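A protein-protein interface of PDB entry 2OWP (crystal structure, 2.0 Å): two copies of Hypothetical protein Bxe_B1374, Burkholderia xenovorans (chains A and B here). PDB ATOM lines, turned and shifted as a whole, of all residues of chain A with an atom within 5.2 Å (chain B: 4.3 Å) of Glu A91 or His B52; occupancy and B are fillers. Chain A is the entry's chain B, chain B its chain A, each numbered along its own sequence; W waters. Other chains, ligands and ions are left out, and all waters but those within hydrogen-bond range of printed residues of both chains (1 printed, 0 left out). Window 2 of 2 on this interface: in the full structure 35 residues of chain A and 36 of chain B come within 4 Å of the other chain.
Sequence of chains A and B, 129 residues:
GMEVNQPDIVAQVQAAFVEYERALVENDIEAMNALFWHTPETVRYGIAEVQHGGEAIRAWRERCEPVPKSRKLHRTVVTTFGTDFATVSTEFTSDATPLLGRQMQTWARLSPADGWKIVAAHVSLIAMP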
ATOM      1  N   LYS A  72      -2.571 -10.881 -17.979  1.00  0.00           N
ATOM      2  CA  LYS A  72      -3.087 -11.761 -19.047  1.00  0.00           C
ATOM      3  C   LYS A  72      -2.428 -13.139 -18.954  1.00  0.00           C
ATOM      4  O   LYS A  72      -1.202 -13.245 -18.926  1.00  0.00           O
ATOM      5  CB  LYS A  72      -2.759 -11.152 -20.407  1.00  0.00           C
ATOM      6  CG  LYS A  72      -3.498 -11.829 -21.589  1.00  0.00           C
ATOM      7  CD  LYS A  72      -3.083 -11.205 -22.926  1.00  0.00           C
ATOM      8  CE  LYS A  72      -3.911 -11.784 -24.076  1.00  0.00           C
ATOM      9  NZ  LYS A  72      -4.086 -13.264 -23.944  1.00  0.00           N
ATOM     10  N   LEU A  73      -3.230 -14.187 -18.921  1.00  0.00           N
ATOM     11  CA  LEU A  73      -2.717 -15.541 -18.830  1.00  0.00           C
ATOM     12  C   LEU A  73      -2.332 -16.056 -20.203  1.00  0.00           C
ATOM     13  O   LEU A  73      -2.886 -15.597 -21.213  1.00  0.00           O
ATOM     14  CB  LEU A  73      -3.770 -16.454 -18.237  1.00  0.00           C
ATOM     15  CG  LEU A  73      -4.246 -16.133 -16.823  1.00  0.00           C
ATOM     16  CD1 LEU A  73      -5.084 -17.343 -16.330  1.00  0.00           C
ATOM     17  CD2 LEU A  73      -3.091 -15.810 -15.883  1.00  0.00           C
ATOM     18  N   HIS A  74      -1.360 -16.974 -20.223  1.00  0.00           N
ATOM     19  CA  HIS A  74      -0.965 -17.730 -21.405  1.00  0.00           C
ATOM     20  C   HIS A  74      -0.675 -19.177 -21.061  1.00  0.00           C
ATOM     21  O   HIS A  74      -0.157 -19.471 -19.990  1.00  0.00           O
ATOM     22  CB  HIS A  74       0.322 -17.171 -21.968  1.00  0.00           C
ATOM     23  CG  HIS A  74       0.314 -15.686 -22.145  1.00  0.00           C
ATOM     24  ND1 HIS A  74      -0.138 -15.082 -23.298  1.00  0.00           N
ATOM     25  CD2 HIS A  74       0.664 -14.687 -21.303  1.00  0.00           C
ATOM     26  CE1 HIS A  74      -0.034 -13.770 -23.171  1.00  0.00           C
ATOM     27  NE2 HIS A  74       0.464 -13.503 -21.975  1.00  0.00           N
ATOM     28  N   ARG A  75      -0.978 -20.077 -21.986  1.00  0.00           N
ATOM     29  CA  ARG A  75      -0.567 -21.481 -21.880  1.00  0.00           C
ATOM     30  C   ARG A  75      -0.958 -22.145 -20.547  1.00  0.00           C
ATOM     31  O   ARG A  75      -0.151 -22.738 -19.823  1.00  0.00           O
ATOM     32  CB  ARG A  75       0.931 -21.587 -22.167  1.00  0.00           C
ATOM     33  CG  ARG A  75       1.274 -21.272 -23.645  1.00  0.00           C
ATOM     34  CD  ARG A  75       2.778 -21.160 -23.903  1.00  0.00           C
ATOM     35  NE  ARG A  75       3.382 -20.102 -23.094  1.00  0.00           N
ATOM     36  CZ  ARG A  75       3.423 -18.809 -23.417  1.00  0.00           C
ATOM     37  NH1 ARG A  75       2.926 -18.378 -24.558  1.00  0.00           N
ATOM     38  NH2 ARG A  75       3.982 -17.933 -22.586  1.00  0.00           N
ATOM     39  N   VAL A  77      -2.429 -24.933 -18.280  1.00  0.00           N
ATOM     40  CA  VAL A  77      -2.575 -26.380 -18.315  1.00  0.00           C
ATOM     41  C   VAL A  77      -3.287 -26.834 -17.038  1.00  0.00           C
ATOM     42  O   VAL A  77      -2.772 -26.679 -15.931  1.00  0.00           O
ATOM     43  CB  VAL A  77      -1.191 -27.082 -18.479  1.00  0.00           C
ATOM     44  CG1 VAL A  77      -1.318 -28.584 -18.525  1.00  0.00           C
ATOM     45  CG2 VAL A  77      -0.458 -26.573 -19.744  1.00  0.00           C
ATOM     46  N   SER A  89      -1.195 -24.945 -13.981  1.00  0.00           N
ATOM     47  CA  SER A  89       0.015 -24.238 -14.278  1.00  0.00           C
ATOM     48  C   SER A  89      -0.304 -23.213 -15.358  1.00  0.00           C
ATOM     49  O   SER A  89      -0.858 -23.556 -16.407  1.00  0.00           O
ATOM     50  CB  SER A  89       1.080 -25.235 -14.813  1.00  0.00           C
ATOM     51  OG  SER A  89       1.192 -26.369 -13.953  1.00  0.00           O
ATOM     52  N   THR A  90       0.047 -21.959 -15.119  1.00  0.00           N
ATOM     53  CA  THR A  90      -0.071 -20.954 -16.163  1.00  0.00           C
ATOM     54  C   THR A  90       1.098 -19.984 -16.180  1.00  0.00           C
ATOM     55  O   THR A  90       1.812 -19.843 -15.189  1.00  0.00           O
ATOM     56  CB  THR A  90      -1.401 -20.164 -15.980  1.00  0.00           C
ATOM     57  OG1 THR A  90      -1.684 -19.407 -17.171  1.00  0.00           O
ATOM     58  CG2 THR A  90      -1.362 -19.255 -14.719  1.00  0.00           C
ATOM     59  N   GLU A  91       1.311 -19.379 -17.351  1.00  0.00           N
ATOM     60  CA  GLU A  91       2.172 -18.229 -17.484  1.00  0.00           C
ATOM     61  C   GLU A  91       1.286 -17.001 -17.533  1.00  0.00           C
ATOM     62  O   GLU A  91       0.049 -17.109 -17.717  1.00  0.00           O
ATOM     63  CB  GLU A  91       3.034 -18.368 -18.716  1.00  0.00           C
ATOM     64  CG  GLU A  91       3.987 -19.544 -18.578  1.00  0.00           C
ATOM     65  CD  GLU A  91       4.509 -20.033 -19.911  1.00  0.00           C
ATOM     66  OE1 GLU A  91       5.353 -19.317 -20.483  1.00  0.00           O
ATOM     67  OE2 GLU A  91       4.056 -21.104 -20.406  1.00  0.00           O
ATOM     68  N   PHE A  92       1.900 -15.850 -17.283  1.00  0.00           N
ATOM     69  CA  PHE A  92       1.183 -14.602 -17.291  1.00  0.00           C
ATOM     70  C   PHE A  92       2.117 -13.454 -17.594  1.00  0.00           C
ATOM     71  O   PHE A  92       3.332 -13.491 -17.259  1.00  0.00           O
ATOM     72  CB  PHE A  92       0.413 -14.379 -15.968  1.00  0.00           C
ATOM     73  CG  PHE A  92       1.283 -14.317 -14.753  1.00  0.00           C
ATOM     74  CD1 PHE A  92       1.613 -15.458 -14.045  1.00  0.00           C
ATOM     75  CD2 PHE A  92       1.773 -13.114 -14.307  1.00  0.00           C
ATOM     76  CE1 PHE A  92       2.423 -15.377 -12.936  1.00  0.00           C
ATOM     77  CE2 PHE A  92       2.572 -13.044 -13.205  1.00  0.00           C
ATOM     78  CZ  PHE A  92       2.895 -14.158 -12.526  1.00  0.00           C
ATOM     79  N   THR A  93       1.543 -12.448 -18.262  1.00  0.00           N
ATOM     80  CA  THR A  93       2.246 -11.193 -18.566  1.00  0.00           C
ATOM     81  C   THR A  93       1.390 -10.022 -18.101  1.00  0.00           C
ATOM     82  O   THR A  93       0.223 -10.213 -17.755  1.00  0.00           O
ATOM     83  CB  THR A  93       2.535 -11.074 -20.083  1.00  0.00           C
ATOM     84  OG1 THR A  93       1.305 -11.152 -20.824  1.00  0.00           O
ATOM     85  CG2 THR A  93       3.423 -12.216 -20.530  1.00  0.00           C
ATOM     86  N   LEU A 100       8.385 -12.507 -17.691  1.00  0.00           N
ATOM     87  CA  LEU A 100       7.365 -13.542 -17.882  1.00  0.00           C
ATOM     88  C   LEU A 100       7.075 -14.143 -16.551  1.00  0.00           C
ATOM     89  O   LEU A 100       8.009 -14.519 -15.834  1.00  0.00           O
ATOM     90  CB  LEU A 100       7.901 -14.621 -18.824  1.00  0.00           C
ATOM     91  CG  LEU A 100       6.997 -15.837 -19.005  1.00  0.00           C
ATOM     92  CD1 LEU A 100       5.669 -15.455 -19.727  1.00  0.00           C
ATOM     93  CD2 LEU A 100       7.802 -16.897 -19.751  1.00  0.00           C
ATOM     94  N   GLY A 101       5.785 -14.275 -16.221  1.00  0.00           N
ATOM     95  CA  GLY A 101       5.375 -14.838 -14.961  1.00  0.00           C
ATOM     96  C   GLY A 101       4.967 -16.293 -15.097  1.00  0.00           C
ATOM     97  O   GLY A 101       4.452 -16.725 -16.158  1.00  0.00           O
ATOM     98  N   ARG A 102       5.239 -17.057 -14.055  1.00  0.00           N
ATOM     99  CA  ARG A 102       4.813 -18.458 -13.999  1.00  0.00           C
ATOM    100  C   ARG A 102       4.108 -18.649 -12.701  1.00  0.00           C
ATOM    101  O   ARG A 102       4.574 -18.134 -11.694  1.00  0.00           O
ATOM    102  CB  ARG A 102       5.978 -19.424 -13.990  1.00  0.00           C
ATOM    103  CG  ARG A 102       6.784 -19.460 -15.267  1.00  0.00           C
ATOM    104  CD  ARG A 102       7.956 -18.598 -15.178  1.00  0.00           C
ATOM    105  NE  ARG A 102       8.824 -18.866 -14.053  1.00  0.00           N
ATOM    106  CZ  ARG A 102       9.816 -19.749 -14.021  1.00  0.00           C
ATOM    107  NH1 ARG A 102      10.097 -20.491 -15.066  1.00  0.00           N
ATOM    108  NH2 ARG A 102      10.510 -19.912 -12.905  1.00  0.00           N
ATOM    109  N   GLN A 103       3.012 -19.414 -12.725  1.00  0.00           N
ATOM    110  CA  GLN A 103       2.246 -19.689 -11.507  1.00  0.00           C
ATOM    111  C   GLN A 103       1.821 -21.152 -11.537  1.00  0.00           C
ATOM    112  O   GLN A 103       1.208 -21.588 -12.534  1.00  0.00           O
ATOM    113  CB  GLN A 103       1.016 -18.802 -11.473  1.00  0.00           C
ATOM    114  CG  GLN A 103       0.005 -19.152 -10.365  1.00  0.00           C
ATOM    115  CD  GLN A 103      -1.239 -18.312 -10.477  1.00  0.00           C
ATOM    116  OE1 GLN A 103      -1.227 -17.164 -10.080  1.00  0.00           O
ATOM    117  NE2 GLN A 103      -2.318 -18.872 -11.076  1.00  0.00           N
ATOM    118  N   THR B  42       2.601 -33.199 -18.529  1.00  0.00           N
ATOM    119  CA  THR B  42       3.569 -32.809 -17.492  1.00  0.00           C
ATOM    120  C   THR B  42       4.057 -31.386 -17.769  1.00  0.00           C
ATOM    121  O   THR B  42       4.297 -31.022 -18.919  1.00  0.00           O
ATOM    122  CB  THR B  42       4.818 -33.738 -17.493  1.00  0.00           C
ATOM    123  OG1 THR B  42       4.425 -35.113 -17.527  1.00  0.00           O
ATOM    124  CG2 THR B  42       5.701 -33.494 -16.291  1.00  0.00           C
ATOM    125  N   VAL B  43       4.195 -30.604 -16.717  1.00  0.00           N
ATOM    126  CA  VAL B  43       4.740 -29.273 -16.812  1.00  0.00           C
ATOM    127  C   VAL B  43       5.865 -29.044 -15.827  1.00  0.00           C
ATOM    128  O   VAL B  43       5.751 -29.347 -14.628  1.00  0.00           O
ATOM    129  CB  VAL B  43       3.649 -28.196 -16.568  1.00  0.00           C
ATOM    130  CG1 VAL B  43       4.257 -26.775 -16.654  1.00  0.00           C
ATOM    131  CG2 VAL B  43       2.537 -28.372 -17.584  1.00  0.00           C
ATOM    132  N   TYR B  45       8.300 -25.765 -14.677  1.00  0.00           N
ATOM    133  CA  TYR B  45       8.791 -24.383 -14.749  1.00  0.00           C
ATOM    134  C   TYR B  45      10.109 -24.355 -14.036  1.00  0.00           C
ATOM    135  O   TYR B  45      10.169 -24.547 -12.823  1.00  0.00           O
ATOM    136  CB  TYR B  45       7.809 -23.459 -14.036  1.00  0.00           C
ATOM    137  CG  TYR B  45       6.430 -23.331 -14.688  1.00  0.00           C
ATOM    138  CD1 TYR B  45       6.266 -23.425 -16.063  1.00  0.00           C
ATOM    139  CD2 TYR B  45       5.293 -23.027 -13.911  1.00  0.00           C
ATOM    140  CE1 TYR B  45       4.999 -23.234 -16.655  1.00  0.00           C
ATOM    141  CE2 TYR B  45       4.052 -22.847 -14.485  1.00  0.00           C
ATOM    142  CZ  TYR B  45       3.907 -22.935 -15.856  1.00  0.00           C
ATOM    143  OH  TYR B  45       2.690 -22.780 -16.422  1.00  0.00           O
ATOM    144  N   VAL B  50      10.803 -22.958 -19.321  1.00  0.00           N
ATOM    145  CA  VAL B  50       9.455 -23.511 -19.199  1.00  0.00           C
ATOM    146  C   VAL B  50       9.393 -24.711 -20.138  1.00  0.00           C
ATOM    147  O   VAL B  50       9.799 -24.601 -21.297  1.00  0.00           O
ATOM    148  CB  VAL B  50       8.407 -22.488 -19.651  1.00  0.00           C
ATOM    149  CG1 VAL B  50       7.034 -23.091 -19.662  1.00  0.00           C
ATOM    150  CG2 VAL B  50       8.462 -21.218 -18.745  1.00  0.00           C
ATOM    151  N   GLN B  51       8.899 -25.844 -19.641  1.00  0.00           N
ATOM    152  CA  GLN B  51       8.813 -27.079 -20.425  1.00  0.00           C
ATOM    153  C   GLN B  51       7.428 -27.680 -20.301  1.00  0.00           C
ATOM    154  O   GLN B  51       6.951 -27.883 -19.177  1.00  0.00           O
ATOM    155  CB  GLN B  51       9.812 -28.113 -19.906  1.00  0.00           C
ATOM    156  CG  GLN B  51      11.239 -27.832 -20.248  1.00  0.00           C
ATOM    157  CD  GLN B  51      12.117 -27.616 -19.060  1.00  0.00           C
ATOM    158  OE1 GLN B  51      11.782 -27.948 -17.910  1.00  0.00           O
ATOM    159  NE2 GLN B  51      13.258 -27.027 -19.316  1.00  0.00           N
ATOM    160  N   HIS B  52       6.798 -27.969 -21.441  1.00  0.00           N
ATOM    161  CA  HIS B  52       5.487 -28.600 -21.487  1.00  0.00           C
ATOM    162  C   HIS B  52       5.687 -29.992 -22.088  1.00  0.00           C
ATOM    163  O   HIS B  52       6.173 -30.131 -23.223  1.00  0.00           O
ATOM    164  CB  HIS B  52       4.517 -27.758 -22.333  1.00  0.00           C
ATOM    165  CG  HIS B  52       4.194 -26.424 -21.736  1.00  0.00           C
ATOM    166  ND1 HIS B  52       4.737 -25.244 -22.207  1.00  0.00           N
ATOM    167  CD2 HIS B  52       3.395 -26.082 -20.696  1.00  0.00           C
ATOM    168  CE1 HIS B  52       4.267 -24.234 -21.496  1.00  0.00           C
ATOM    169  NE2 HIS B  52       3.455 -24.717 -20.569  1.00  0.00           N
ATOM    170  N   GLY B  53       5.382 -31.019 -21.305  1.00  0.00           N
ATOM    171  CA  GLY B  53       5.476 -32.395 -21.758  1.00  0.00           C
ATOM    172  C   GLY B  53       6.760 -33.091 -21.344  1.00  0.00           C
ATOM    173  O   GLY B  53       7.838 -32.495 -21.350  1.00  0.00           O
ATOM    174  N   ALA B  56      10.035 -32.725 -23.723  1.00  0.00           N
ATOM    175  CA  ALA B  56      10.809 -31.492 -23.609  1.00  0.00           C
ATOM    176  C   ALA B  56      11.648 -31.540 -22.359  1.00  0.00           C
ATOM    177  O   ALA B  56      12.838 -31.164 -22.379  1.00  0.00           O
ATOM    178  CB  ALA B  56       9.892 -30.277 -23.607  1.00  0.00           C
HETATM  179  O   HOH W   1       2.515 -22.736 -19.313  1.00  0.00           O
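O of Thr A90 sits at hydrogen-bond distance from N of Gln A103, 2.8 Å away. The guanidinium group (NH2) of Arg A75 is in salt-bridge range of the side-chain carboxylate (OE1) of Glu A91 (2.9 Å). O of His A74 is in hydrogen-bond range of OG1 of Thr A90, at 3.2 Å. The backbone NH (N) of His A74 lies within hydrogen-bond range of the backbone carbonyl oxygen (O) of Glu A91 (2.9 Å). N of Val A77 is in hydrogen-bond range of O of Ser A89, at 2.8 Å.
No position is printed for both chains.
Water W1 lies within hydrogen-bond range of OE2 of Glu A91, NE2 of His B52, O of Arg A75 and OH of Tyr B45.
Among the printed residues, merely in contact across the chains: Ser A89 with Tyr B45, Glu A91 with His B52, Glu A91 with Val B50, Arg A102 with Tyr B45, Gln A103 with Tyr B45, Glu A91 with Tyr B45, Val A77 with Val B43, Ser A89 with Val B43 and Val A77 with His B52.
Hydrophobic or aromatic side chains of chain B that line the printed part of chain A: Val B43, Tyr B45, Val B50 and His B52. Among the printed residues, no Asp or Glu carboxylate lies within 4 Å of a Lys or Arg side-chain nitrogen of the other chain.
Printed residues of chain B within 4 Å of Ser A89: Val B43 (3.98 Å) and Tyr B45 (3.2 Å). Of chain B, only Tyr B45, Val B50 and His B52 come within 4 Å of Glu A91. Of the printed residues of chain A, Val B43 touches Val A77 (3.97 Å) and Ser A89 (3.98 Å). Printed residues of chain A within 4 Å of Val B50: Glu A91. Of the printed residues of chain A, His B52 touches Val A77 and Glu A91. The nearest printed residue of chain B that does not touch Glu A91 is Val B43 (6.8 Å). The nearest printed residue of chain A that does not touch His B52 is Arg A75 (4.2 Å). The nearest printed residue of chain A that does not touch Val B43 is Thr A90 (6.6 Å).
OH of Tyr B45 lies within hydrogen-bond range of N of Thr A90, 3.1 Å away.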
